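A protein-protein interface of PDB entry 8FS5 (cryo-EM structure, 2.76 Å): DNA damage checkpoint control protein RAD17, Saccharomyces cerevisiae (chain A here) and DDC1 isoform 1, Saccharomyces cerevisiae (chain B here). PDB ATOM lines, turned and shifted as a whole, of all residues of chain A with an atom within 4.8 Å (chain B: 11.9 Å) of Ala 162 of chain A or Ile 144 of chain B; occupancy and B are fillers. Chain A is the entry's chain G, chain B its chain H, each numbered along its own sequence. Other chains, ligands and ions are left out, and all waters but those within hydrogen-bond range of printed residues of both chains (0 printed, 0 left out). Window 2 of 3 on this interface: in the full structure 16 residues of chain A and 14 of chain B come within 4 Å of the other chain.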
ATOM      1  N   LYS A 159      24.491 -13.298 -21.822  1.00  0.00           N
ATOM      2  CA  LYS A 159      24.574 -13.775 -20.453  1.00  0.00           C
ATOM      3  C   LYS A 159      24.935 -15.260 -20.429  1.00  0.00           C
ATOM      4  O   LYS A 159      24.814 -15.976 -21.426  1.00  0.00           O
ATOM      5  CB  LYS A 159      23.256 -13.533 -19.719  1.00  0.00           C
ATOM      6  CG  LYS A 159      23.316 -12.422 -18.681  1.00  0.00           C
ATOM      7  CD  LYS A 159      22.141 -12.487 -17.710  1.00  0.00           C
ATOM      8  CE  LYS A 159      21.768 -13.922 -17.362  1.00  0.00           C
ATOM      9  NZ  LYS A 159      20.803 -13.986 -16.230  1.00  0.00           N
ATOM     10  N   GLY A 160      25.382 -15.721 -19.264  1.00  0.00           N
ATOM     11  CA  GLY A 160      25.809 -17.099 -19.119  1.00  0.00           C
ATOM     12  C   GLY A 160      24.671 -18.086 -18.967  1.00  0.00           C
ATOM     13  O   GLY A 160      24.690 -19.160 -19.576  1.00  0.00           O
ATOM     14  N   GLU A 161      23.671 -17.733 -18.153  1.00  0.00           N
ATOM     15  CA  GLU A 161      22.545 -18.628 -17.913  1.00  0.00           C
ATOM     16  C   GLU A 161      21.723 -18.887 -19.167  1.00  0.00           C
ATOM     17  O   GLU A 161      21.336 -20.036 -19.412  1.00  0.00           O
ATOM     18  CB  GLU A 161      21.645 -18.059 -16.815  1.00  0.00           C
ATOM     19  CG  GLU A 161      22.260 -18.089 -15.426  1.00  0.00           C
ATOM     20  CD  GLU A 161      21.282 -18.555 -14.367  1.00  0.00           C
ATOM     21  OE1 GLU A 161      21.212 -19.777 -14.116  1.00  0.00           O
ATOM     22  OE2 GLU A 161      20.581 -17.701 -13.784  1.00  0.00           O
ATOM     23  N   ALA A 162      21.448 -17.852 -19.964  1.00  0.00           N
ATOM     24  CA  ALA A 162      20.659 -18.024 -21.184  1.00  0.00           C
ATOM     25  C   ALA A 162      21.387 -18.916 -22.186  1.00  0.00           C
ATOM     26  O   ALA A 162      20.786 -19.812 -22.790  1.00  0.00           O
ATOM     27  CB  ALA A 162      20.341 -16.657 -21.796  1.00  0.00           C
ATOM     28  N   LEU A 163      22.689 -18.682 -22.370  1.00  0.00           N
ATOM     29  CA  LEU A 163      23.469 -19.516 -23.279  1.00  0.00           C
ATOM     30  C   LEU A 163      23.563 -20.950 -22.781  1.00  0.00           C
ATOM     31  O   LEU A 163      23.486 -21.889 -23.581  1.00  0.00           O
ATOM     32  CB  LEU A 163      24.867 -18.928 -23.468  1.00  0.00           C
ATOM     33  CG  LEU A 163      25.683 -19.549 -24.603  1.00  0.00           C
ATOM     34  CD1 LEU A 163      24.906 -19.506 -25.910  1.00  0.00           C
ATOM     35  CD2 LEU A 163      27.021 -18.849 -24.748  1.00  0.00           C
ATOM     36  N   HIS A 164      23.732 -21.141 -21.470  1.00  0.00           N
ATOM     37  CA  HIS A 164      23.764 -22.491 -20.917  1.00  0.00           C
ATOM     38  C   HIS A 164      22.440 -23.215 -21.124  1.00  0.00           C
ATOM     39  O   HIS A 164      22.434 -24.399 -21.483  1.00  0.00           O
ATOM     40  CB  HIS A 164      24.118 -22.443 -19.432  1.00  0.00           C
ATOM     41  CG  HIS A 164      24.191 -23.790 -18.784  1.00  0.00           C
ATOM     42  ND1 HIS A 164      25.264 -24.639 -18.952  1.00  0.00           N
ATOM     43  CD2 HIS A 164      23.323 -24.436 -17.969  1.00  0.00           C
ATOM     44  CE1 HIS A 164      25.054 -25.750 -18.268  1.00  0.00           C
ATOM     45  NE2 HIS A 164      23.884 -25.651 -17.662  1.00  0.00           N
ATOM     46  N   SER A 165      21.317 -22.526 -20.910  1.00  0.00           N
ATOM     47  CA  SER A 165      20.010 -23.130 -21.148  1.00  0.00           C
ATOM     48  C   SER A 165      19.810 -23.470 -22.620  1.00  0.00           C
ATOM     49  O   SER A 165      19.272 -24.535 -22.945  1.00  0.00           O
ATOM     50  CB  SER A 165      18.903 -22.194 -20.659  1.00  0.00           C
ATOM     51  OG  SER A 165      18.874 -20.999 -21.420  1.00  0.00           O
ATOM     52  N   ALA A 166      20.235 -22.580 -23.520  1.00  0.00           N
ATOM     53  CA  ALA A 166      20.121 -22.859 -24.949  1.00  0.00           C
ATOM     54  C   ALA A 166      20.965 -24.065 -25.348  1.00  0.00           C
ATOM     55  O   ALA A 166      20.515 -24.911 -26.130  1.00  0.00           O
ATOM     56  CB  ALA A 166      20.526 -21.628 -25.758  1.00  0.00           C
ATOM     57  N   ILE A 205      16.329 -21.454 -31.528  1.00  0.00           N
ATOM     58  CA  ILE A 205      16.291 -20.833 -30.208  1.00  0.00           C
ATOM     59  C   ILE A 205      16.665 -19.370 -30.381  1.00  0.00           C
ATOM     60  O   ILE A 205      17.776 -19.057 -30.828  1.00  0.00           O
ATOM     61  CB  ILE A 205      17.238 -21.527 -29.217  1.00  0.00           C
ATOM     62  CG1 ILE A 205      16.896 -23.013 -29.102  1.00  0.00           C
ATOM     63  CG2 ILE A 205      17.171 -20.852 -27.855  1.00  0.00           C
ATOM     64  CD1 ILE A 205      17.731 -23.752 -28.079  1.00  0.00           C
ATOM     65  N   LYS A 206      15.750 -18.474 -30.020  1.00  0.00           N
ATOM     66  CA  LYS A 206      15.922 -17.041 -30.228  1.00  0.00           C
ATOM     67  C   LYS A 206      16.263 -16.370 -28.905  1.00  0.00           C
ATOM     68  O   LYS A 206      15.445 -16.367 -27.978  1.00  0.00           O
ATOM     69  CB  LYS A 206      14.661 -16.422 -30.830  1.00  0.00           C
ATOM     70  CG  LYS A 206      14.745 -16.165 -32.324  1.00  0.00           C
ATOM     71  CD  LYS A 206      15.216 -14.749 -32.611  1.00  0.00           C
ATOM     72  CE  LYS A 206      14.232 -13.721 -32.075  1.00  0.00           C
ATOM     73  NZ  LYS A 206      14.865 -12.386 -31.901  1.00  0.00           N
ATOM     74  N   LEU A 207      17.460 -15.807 -28.822  1.00  0.00           N
ATOM     75  CA  LEU A 207      17.828 -15.010 -27.658  1.00  0.00           C
ATOM     76  C   LEU A 207      17.089 -13.677 -27.702  1.00  0.00           C
ATOM     77  O   LEU A 207      16.958 -13.083 -28.779  1.00  0.00           O
ATOM     78  CB  LEU A 207      19.339 -14.783 -27.603  1.00  0.00           C
ATOM     79  CG  LEU A 207      20.233 -15.928 -27.110  1.00  0.00           C
ATOM     80  CD1 LEU A 207      19.717 -16.480 -25.787  1.00  0.00           C
ATOM     81  CD2 LEU A 207      20.383 -17.042 -28.142  1.00  0.00           C
ATOM     82  N   PRO A 208      16.588 -13.184 -26.571  1.00  0.00           N
ATOM     83  CA  PRO A 208      15.815 -11.936 -26.586  1.00  0.00           C
ATOM     84  C   PRO A 208      16.677 -10.740 -26.963  1.00  0.00           C
ATOM     85  O   PRO A 208      17.887 -10.722 -26.732  1.00  0.00           O
ATOM     86  CB  PRO A 208      15.295 -11.818 -25.148  1.00  0.00           C
ATOM     87  CG  PRO A 208      15.483 -13.171 -24.540  1.00  0.00           C
ATOM     88  CD  PRO A 208      16.647 -13.787 -25.232  1.00  0.00           C
ATOM     89  N   ILE A 213      19.787 -10.022 -21.423  1.00  0.00           N
ATOM     90  CA  ILE A 213      20.266 -11.280 -21.986  1.00  0.00           C
ATOM     91  C   ILE A 213      21.298 -10.984 -23.065  1.00  0.00           C
ATOM     92  O   ILE A 213      22.438 -11.455 -22.997  1.00  0.00           O
ATOM     93  CB  ILE A 213      19.107 -12.120 -22.548  1.00  0.00           C
ATOM     94  CG1 ILE A 213      18.138 -12.509 -21.430  1.00  0.00           C
ATOM     95  CG2 ILE A 213      19.646 -13.352 -23.253  1.00  0.00           C
ATOM     96  CD1 ILE A 213      18.762 -13.367 -20.352  1.00  0.00           C
ATOM     97  N   ILE B 104       9.979 -31.561 -26.653  1.00  0.00           N
ATOM     98  CA  ILE B 104       9.515 -30.189 -26.809  1.00  0.00           C
ATOM     99  C   ILE B 104       8.687 -29.752 -25.613  1.00  0.00           C
ATOM    100  O   ILE B 104       8.889 -28.653 -25.085  1.00  0.00           O
ATOM    101  CB  ILE B 104       8.700 -30.034 -28.108  1.00  0.00           C
ATOM    102  CG1 ILE B 104       9.511 -30.483 -29.321  1.00  0.00           C
ATOM    103  CG2 ILE B 104       8.263 -28.595 -28.287  1.00  0.00           C
ATOM    104  CD1 ILE B 104       8.740 -30.379 -30.618  1.00  0.00           C
ATOM    105  N   ARG B 106       8.815 -31.039 -22.683  1.00  0.00           N
ATOM    106  CA  ARG B 106       9.573 -31.197 -21.449  1.00  0.00           C
ATOM    107  C   ARG B 106       9.842 -29.839 -20.816  1.00  0.00           C
ATOM    108  O   ARG B 106      10.247 -28.893 -21.494  1.00  0.00           O
ATOM    109  CB  ARG B 106      10.891 -31.919 -21.732  1.00  0.00           C
ATOM    110  CG  ARG B 106      11.708 -32.233 -20.487  1.00  0.00           C
ATOM    111  CD  ARG B 106      12.648 -33.406 -20.719  1.00  0.00           C
ATOM    112  NE  ARG B 106      12.195 -34.616 -20.045  1.00  0.00           N
ATOM    113  CZ  ARG B 106      11.579 -35.623 -20.649  1.00  0.00           C
ATOM    114  NH1 ARG B 106      11.326 -35.601 -21.948  1.00  0.00           N
ATOM    115  NH2 ARG B 106      11.209 -36.682 -19.933  1.00  0.00           N
ATOM    116  N   PRO B 108      12.041 -27.399 -18.992  1.00  0.00           N
ATOM    117  CA  PRO B 108      13.469 -27.273 -18.692  1.00  0.00           C
ATOM    118  C   PRO B 108      13.705 -26.880 -17.241  1.00  0.00           C
ATOM    119  O   PRO B 108      12.866 -26.259 -16.586  1.00  0.00           O
ATOM    120  CB  PRO B 108      13.941 -26.174 -19.653  1.00  0.00           C
ATOM    121  CG  PRO B 108      12.896 -26.138 -20.728  1.00  0.00           C
ATOM    122  CD  PRO B 108      11.616 -26.427 -20.010  1.00  0.00           C
ATOM    123  N   ASP B 109      14.876 -27.260 -16.745  1.00  0.00           N
ATOM    124  CA  ASP B 109      15.282 -26.994 -15.369  1.00  0.00           C
ATOM    125  C   ASP B 109      15.951 -25.623 -15.330  1.00  0.00           C
ATOM    126  O   ASP B 109      16.953 -25.389 -16.010  1.00  0.00           O
ATOM    127  CB  ASP B 109      16.212 -28.094 -14.870  1.00  0.00           C
ATOM    128  CG  ASP B 109      17.084 -27.646 -13.716  1.00  0.00           C
ATOM    129  OD1 ASP B 109      16.559 -27.032 -12.763  1.00  0.00           O
ATOM    130  OD2 ASP B 109      18.302 -27.903 -13.774  1.00  0.00           O
ATOM    131  N   GLY B 110      15.391 -24.719 -14.532  1.00  0.00           N
ATOM    132  CA  GLY B 110      15.932 -23.379 -14.375  1.00  0.00           C
ATOM    133  C   GLY B 110      15.238 -22.306 -15.189  1.00  0.00           C
ATOM    134  O   GLY B 110      15.551 -21.122 -15.005  1.00  0.00           O
ATOM    135  N   ASP B 111      14.311 -22.650 -16.083  1.00  0.00           N
ATOM    136  CA  ASP B 111      13.623 -21.650 -16.898  1.00  0.00           C
ATOM    137  C   ASP B 111      12.222 -22.181 -17.192  1.00  0.00           C
ATOM    138  O   ASP B 111      12.061 -23.094 -18.006  1.00  0.00           O
ATOM    139  CB  ASP B 111      14.395 -21.360 -18.178  1.00  0.00           C
ATOM    140  CG  ASP B 111      14.503 -19.877 -18.471  1.00  0.00           C
ATOM    141  OD1 ASP B 111      14.180 -19.067 -17.577  1.00  0.00           O
ATOM    142  OD2 ASP B 111      14.910 -19.520 -19.597  1.00  0.00           O
ATOM    143  N   GLY B 112      11.222 -21.608 -16.526  1.00  0.00           N
ATOM    144  CA  GLY B 112       9.860 -22.067 -16.701  1.00  0.00           C
ATOM    145  C   GLY B 112       9.248 -21.602 -18.008  1.00  0.00           C
ATOM    146  O   GLY B 112       9.780 -20.749 -18.720  1.00  0.00           O
ATOM    147  N   ILE B 113       8.095 -22.185 -18.323  1.00  0.00           N
ATOM    148  CA  ILE B 113       7.368 -21.873 -19.548  1.00  0.00           C
ATOM    149  C   ILE B 113       6.274 -20.861 -19.238  1.00  0.00           C
ATOM    150  O   ILE B 113       5.501 -21.037 -18.288  1.00  0.00           O
ATOM    151  CB  ILE B 113       6.774 -23.145 -20.175  1.00  0.00           C
ATOM    152  CG1 ILE B 113       7.739 -24.322 -20.014  1.00  0.00           C
ATOM    153  CG2 ILE B 113       6.424 -22.908 -21.640  1.00  0.00           C
ATOM    154  CD1 ILE B 113       8.857 -24.335 -21.030  1.00  0.00           C
ATOM    155  N   LYS B 114       6.209 -19.801 -20.040  1.00  0.00           N
ATOM    156  CA  LYS B 114       5.161 -18.797 -19.916  1.00  0.00           C
ATOM    157  C   LYS B 114       4.021 -19.004 -20.903  1.00  0.00           C
ATOM    158  O   LYS B 114       2.854 -18.881 -20.519  1.00  0.00           O
ATOM    159  CB  LYS B 114       5.749 -17.393 -20.106  1.00  0.00           C
ATOM    160  CG  LYS B 114       4.727 -16.312 -20.422  1.00  0.00           C
ATOM    161  CD  LYS B 114       5.366 -14.932 -20.439  1.00  0.00           C
ATOM    162  CE  LYS B 114       6.538 -14.875 -21.404  1.00  0.00           C
ATOM    163  NZ  LYS B 114       6.187 -14.170 -22.668  1.00  0.00           N
ATOM    164  N   SER B 115       4.329 -19.332 -22.156  1.00  0.00           N
ATOM    165  CA  SER B 115       3.299 -19.552 -23.169  1.00  0.00           C
ATOM    166  C   SER B 115       3.738 -20.710 -24.053  1.00  0.00           C
ATOM    167  O   SER B 115       4.743 -20.603 -24.761  1.00  0.00           O
ATOM    168  CB  SER B 115       3.065 -18.289 -23.996  1.00  0.00           C
ATOM    169  OG  SER B 115       2.881 -17.158 -23.163  1.00  0.00           O
ATOM    170  N   PHE B 116       2.988 -21.808 -24.011  1.00  0.00           N
ATOM    171  CA  PHE B 116       3.231 -22.966 -24.864  1.00  0.00           C
ATOM    172  C   PHE B 116       2.164 -22.981 -25.953  1.00  0.00           C
ATOM    173  O   PHE B 116       1.011 -23.340 -25.697  1.00  0.00           O
ATOM    174  CB  PHE B 116       3.212 -24.259 -24.053  1.00  0.00           C
ATOM    175  CG  PHE B 116       3.427 -25.499 -24.877  1.00  0.00           C
ATOM    176  CD1 PHE B 116       4.708 -25.913 -25.206  1.00  0.00           C
ATOM    177  CD2 PHE B 116       2.350 -26.256 -25.312  1.00  0.00           C
ATOM    178  CE1 PHE B 116       4.910 -27.055 -25.958  1.00  0.00           C
ATOM    179  CE2 PHE B 116       2.547 -27.397 -26.067  1.00  0.00           C
ATOM    180  CZ  PHE B 116       3.827 -27.797 -26.391  1.00  0.00           C
ATOM    181  N   THR B 117       2.553 -22.599 -27.165  1.00  0.00           N
ATOM    182  CA  THR B 117       1.642 -22.502 -28.297  1.00  0.00           C
ATOM    183  C   THR B 117       1.875 -23.674 -29.238  1.00  0.00           C
ATOM    184  O   THR B 117       3.017 -23.956 -29.610  1.00  0.00           O
ATOM    185  CB  THR B 117       1.838 -21.178 -29.042  1.00  0.00           C
ATOM    186  OG1 THR B 117       1.357 -20.095 -28.235  1.00  0.00           O
ATOM    187  CG2 THR B 117       1.093 -21.187 -30.369  1.00  0.00           C
ATOM    188  N   VAL B 136       5.131 -25.512 -33.036  1.00  0.00           N
ATOM    189  CA  VAL B 136       5.008 -25.380 -31.590  1.00  0.00           C
ATOM    190  C   VAL B 136       5.909 -24.234 -31.144  1.00  0.00           C
ATOM    191  O   VAL B 136       7.087 -24.180 -31.520  1.00  0.00           O
ATOM    192  CB  VAL B 136       5.355 -26.689 -30.862  1.00  0.00           C
ATOM    193  CG1 VAL B 136       6.565 -27.356 -31.494  1.00  0.00           C
ATOM    194  CG2 VAL B 136       5.582 -26.432 -29.382  1.00  0.00           C
ATOM    195  N   VAL B 137       5.353 -23.318 -30.353  1.00  0.00           N
ATOM    196  CA  VAL B 137       6.050 -22.116 -29.911  1.00  0.00           C
ATOM    197  C   VAL B 137       6.194 -22.168 -28.397  1.00  0.00           C
ATOM    198  O   VAL B 137       5.208 -22.377 -27.680  1.00  0.00           O
ATOM    199  CB  VAL B 137       5.301 -20.842 -30.340  1.00  0.00           C
ATOM    200  CG1 VAL B 137       6.030 -19.599 -29.848  1.00  0.00           C
ATOM    201  CG2 VAL B 137       5.119 -20.809 -31.848  1.00  0.00           C
ATOM    202  N   ILE B 138       7.419 -21.977 -27.914  1.00  0.00           N
ATOM    203  CA  ILE B 138       7.708 -21.905 -26.486  1.00  0.00           C
ATOM    204  C   ILE B 138       8.345 -20.553 -26.201  1.00  0.00           C
ATOM    205  O   ILE B 138       9.371 -20.204 -26.800  1.00  0.00           O
ATOM    206  CB  ILE B 138       8.625 -23.048 -26.023  1.00  0.00           C
ATOM    207  CG1 ILE B 138       8.062 -24.400 -26.461  1.00  0.00           C
ATOM    208  CG2 ILE B 138       8.810 -23.003 -24.516  1.00  0.00           C
ATOM    209  CD1 ILE B 138       9.008 -25.553 -26.233  1.00  0.00           C
ATOM    210  N   GLU B 139       7.742 -19.796 -25.290  1.00  0.00           N
ATOM    211  CA  GLU B 139       8.261 -18.504 -24.847  1.00  0.00           C
ATOM    212  C   GLU B 139       8.541 -18.616 -23.351  1.00  0.00           C
ATOM    213  O   GLU B 139       7.621 -18.697 -22.535  1.00  0.00           O
ATOM    214  CB  GLU B 139       7.280 -17.376 -25.158  1.00  0.00           C
ATOM    215  CG  GLU B 139       6.735 -17.400 -26.576  1.00  0.00           C
ATOM    216  CD  GLU B 139       5.241 -17.151 -26.630  1.00  0.00           C
ATOM    217  OE1 GLU B 139       4.503 -18.050 -27.087  1.00  0.00           O
ATOM    218  OE2 GLU B 139       4.804 -16.057 -26.215  1.00  0.00           O
ATOM    219  N   MET B 140       9.823 -18.624 -22.998  1.00  0.00           N
ATOM    220  CA  MET B 140      10.221 -18.779 -21.608  1.00  0.00           C
ATOM    221  C   MET B 140       9.953 -17.497 -20.825  1.00  0.00           C
ATOM    222  O   MET B 140       9.756 -16.418 -21.392  1.00  0.00           O
ATOM    223  CB  MET B 140      11.703 -19.143 -21.519  1.00  0.00           C
ATOM    224  CG  MET B 140      12.131 -20.227 -22.492  1.00  0.00           C
ATOM    225  SD  MET B 140      11.441 -21.841 -22.097  1.00  0.00           S
ATOM    226  CE  MET B 140      12.834 -22.584 -21.257  1.00  0.00           C
ATOM    227  N   ASP B 141       9.947 -17.627 -19.497  1.00  0.00           N
ATOM    228  CA  ASP B 141       9.838 -16.454 -18.637  1.00  0.00           C
ATOM    229  C   ASP B 141      11.064 -15.557 -18.726  1.00  0.00           C
ATOM    230  O   ASP B 141      10.978 -14.379 -18.358  1.00  0.00           O
ATOM    231  CB  ASP B 141       9.607 -16.880 -17.185  1.00  0.00           C
ATOM    232  CG  ASP B 141      10.347 -18.151 -16.824  1.00  0.00           C
ATOM    233  OD1 ASP B 141      11.410 -18.412 -17.423  1.00  0.00           O
ATOM    234  OD2 ASP B 141       9.866 -18.887 -15.937  1.00  0.00           O
ATOM    235  N   SER B 142      12.194 -16.078 -19.199  1.00  0.00           N
ATOM    236  CA  SER B 142      13.369 -15.276 -19.503  1.00  0.00           C
ATOM    237  C   SER B 142      13.315 -14.674 -20.903  1.00  0.00           C
ATOM    238  O   SER B 142      14.358 -14.288 -21.440  1.00  0.00           O
ATOM    239  CB  SER B 142      14.639 -16.118 -19.345  1.00  0.00           C
ATOM    240  OG  SER B 142      14.680 -17.165 -20.300  1.00  0.00           O
ATOM    241  N   LEU B 143      12.124 -14.605 -21.502  1.00  0.00           N
ATOM    242  CA  LEU B 143      11.838 -14.056 -22.826  1.00  0.00           C
ATOM    243  C   LEU B 143      12.525 -14.811 -23.957  1.00  0.00           C
ATOM    244  O   LEU B 143      12.494 -14.340 -25.100  1.00  0.00           O
ATOM    245  CB  LEU B 143      12.191 -12.563 -22.946  1.00  0.00           C
ATOM    246  CG  LEU B 143      11.518 -11.520 -22.039  1.00  0.00           C
ATOM    247  CD1 LEU B 143      10.001 -11.684 -22.061  1.00  0.00           C
ATOM    248  CD2 LEU B 143      12.057 -11.499 -20.608  1.00  0.00           C
ATOM    249  N   ILE B 144      13.135 -15.962 -23.691  1.00  0.00           N
ATOM    250  CA  ILE B 144      13.767 -16.754 -24.741  1.00  0.00           C
ATOM    251  C   ILE B 144      12.678 -17.472 -25.527  1.00  0.00           C
ATOM    252  O   ILE B 144      11.828 -18.155 -24.948  1.00  0.00           O
ATOM    253  CB  ILE B 144      14.777 -17.750 -24.154  1.00  0.00           C
ATOM    254  CG1 ILE B 144      15.913 -17.005 -23.449  1.00  0.00           C
ATOM    255  CG2 ILE B 144      15.325 -18.659 -25.245  1.00  0.00           C
ATOM    256  CD1 ILE B 144      17.055 -17.898 -23.015  1.00  0.00           C
ATOM    257  N   VAL B 145      12.698 -17.316 -26.847  1.00  0.00           N
ATOM    258  CA  VAL B 145      11.717 -17.933 -27.729  1.00  0.00           C
ATOM    259  C   VAL B 145      12.369 -19.132 -28.402  1.00  0.00           C
ATOM    260  O   VAL B 145      13.353 -18.984 -29.137  1.00  0.00           O
ATOM    261  CB  VAL B 145      11.188 -16.934 -28.769  1.00  0.00           C
ATOM    262  CG1 VAL B 145      10.233 -17.626 -29.730  1.00  0.00           C
ATOM    263  CG2 VAL B 145      10.504 -15.765 -28.080  1.00  0.00           C
ATOM    264  N   LYS B 146      11.822 -20.319 -28.155  1.00  0.00           N
ATOM    265  CA  LYS B 146      12.329 -21.555 -28.736  1.00  0.00           C
ATOM    266  C   LYS B 146      11.338 -22.053 -29.782  1.00  0.00           C
ATOM    267  O   LYS B 146      10.151 -22.225 -29.486  1.00  0.00           O
ATOM    268  CB  LYS B 146      12.562 -22.610 -27.655  1.00  0.00           C
ATOM    269  CG  LYS B 146      13.183 -22.057 -26.380  1.00  0.00           C
ATOM    270  CD  LYS B 146      13.512 -23.157 -25.381  1.00  0.00           C
ATOM    271  CE  LYS B 146      12.368 -24.147 -25.234  1.00  0.00           C
ATOM    272  NZ  LYS B 146      12.670 -25.187 -24.212  1.00  0.00           N
ATOM    273  N   GLU B 147      11.830 -22.282 -30.996  1.00  0.00           N
ATOM    274  CA  GLU B 147      11.008 -22.690 -32.125  1.00  0.00           C
ATOM    275  C   GLU B 147      11.328 -24.130 -32.501  1.00  0.00           C
ATOM    276  O   GLU B 147      12.496 -24.532 -32.516  1.00  0.00           O
ATOM    277  CB  GLU B 147      11.244 -21.773 -33.337  1.00  0.00           C
ATOM    278  CG  GLU B 147      10.094 -20.829 -33.713  1.00  0.00           C
ATOM    279  CD  GLU B 147       8.722 -21.490 -33.805  1.00  0.00           C
ATOM    280  OE1 GLU B 147       7.719 -20.753 -33.711  1.00  0.00           O
ATOM    281  OE2 GLU B 147       8.629 -22.716 -34.029  1.00  0.00           O
ATOM    282  N   TYR B 148      10.287 -24.903 -32.798  1.00  0.00           N
ATOM    283  CA  TYR B 148      10.434 -26.280 -33.246  1.00  0.00           C
ATOM    284  C   TYR B 148       9.504 -26.525 -34.425  1.00  0.00           C
ATOM    285  O   TYR B 148       8.425 -25.932 -34.507  1.00  0.00           O
ATOM    286  CB  TYR B 148      10.119 -27.280 -32.126  1.00  0.00           C
ATOM    287  CG  TYR B 148      10.992 -27.145 -30.899  1.00  0.00           C
ATOM    288  CD1 TYR B 148      10.663 -26.257 -29.883  1.00  0.00           C
ATOM    289  CD2 TYR B 148      12.136 -27.918 -30.750  1.00  0.00           C
ATOM    290  CE1 TYR B 148      11.455 -26.136 -28.759  1.00  0.00           C
ATOM    291  CE2 TYR B 148      12.933 -27.803 -29.629  1.00  0.00           C
ATOM    292  CZ  TYR B 148      12.587 -26.911 -28.637  1.00  0.00           C
ATOM    293  OH  TYR B 148      13.377 -26.793 -27.518  1.00  0.00           O
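No residue of chain B comes within 4 Å of Lys 159 of chain A.
No residue of chain B comes within 4 Å of Gly 160 of chain A.
No residue of chain B comes within 4 Å of Glu 161 of chain A.
Of chain B, only Ile 144 comes within 4 Å of Ala 162 of chain A.
No residue of chain B comes within 4 Å of Leu 163 of chain A.
Printed residues of chain B within 4 Å of Ile 205 of chain A: Ile 144 and Val 145.
Of the printed residues of chain B, Lys 206 of chain A touches Ile 144 and Val 145.
No residue of chain B comes within 4 Å of Leu 207 of chain A.
Pro 208 of chain A touches just these residues of chain B: Ser 142, Leu 143 and Ile 144.
No residue of chain B comes within 4 Å of Ile 213 of chain A.
Asp 111 of chain B touches none of the printed residues of chain A.
Printed residues of chain A within 4 Å of Ser 142 of chain B: Pro 208.
Printed residues of chain A within 4 Å of Leu 143 of chain B: Pro 208.
Ile 144 of chain B touches five residues of chain A.
Of the printed residues of chain A, Val 145 of chain B touches Ile 205 and Lys 206.
The nearest residue of chain B that does not touch Ala 162 of chain A is Ser 142 of chain B (5.9 Å).
The nearest residue of chain A that does not touch Ile 144 of chain B is Leu 207 of chain A (4.1 Å).
Of the 25 printed residues of chain B, 4 touch a printed residue of chain A.
Printed residues of chain A that touch a printed residue of chain B: Ala 162, Ser 165, Ile 205, Lys 206 and Pro 208.
Hydrophobic or aromatic side chains of chain A within 4 Å of the printed part of chain B: Ala 162, Ile 205 and Pro 208.
Among the printed residues, 9 pairs touch across the chains.
The backbone carbonyl oxygen (O) of Glu 161 of chain A is in hydrogen-bond range of the side-chain hydroxyl (OG) of Ser 165 of chain A (3.3 Å).
O of Ala 162 of chain A sits at hydrogen-bond distance from OG of Ser 165 of chain A (2.6 Å).
OD2 of Asp 111 of chain B sits at hydrogen-bond distance from OG of Ser 142 of chain B (2.5 Å).
Ala 162 of chain A touches Ile 144 of chain B (CB to CD1, 3.7 Å).
OG of Ser 165 of chain A touches CD1 of Ile 144 of chain B, at 3.9 Å.
Ile 205 of chain A touches Ile 144 of chain B (CG2 to CG2, 3.9 Å).
Val 145 of chain B touches Ile 205 of chain A.
Ile 144 of chain B touches Lys 206 of chain A.
Pro 208 of chain A touches Ser 142 of chain B (CG to O, 3.5 Å).
Pro 208 of chain A touches Leu 143 of chain B (CG to O, 3.3 Å).
Pro 208 of chain A touches Ile 144 of chain B (CG to N, 3.7 Å).
N of Lys 206 of chain A sits at hydrogen-bond distance from O of Val 145 of chain B (2.6 Å).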
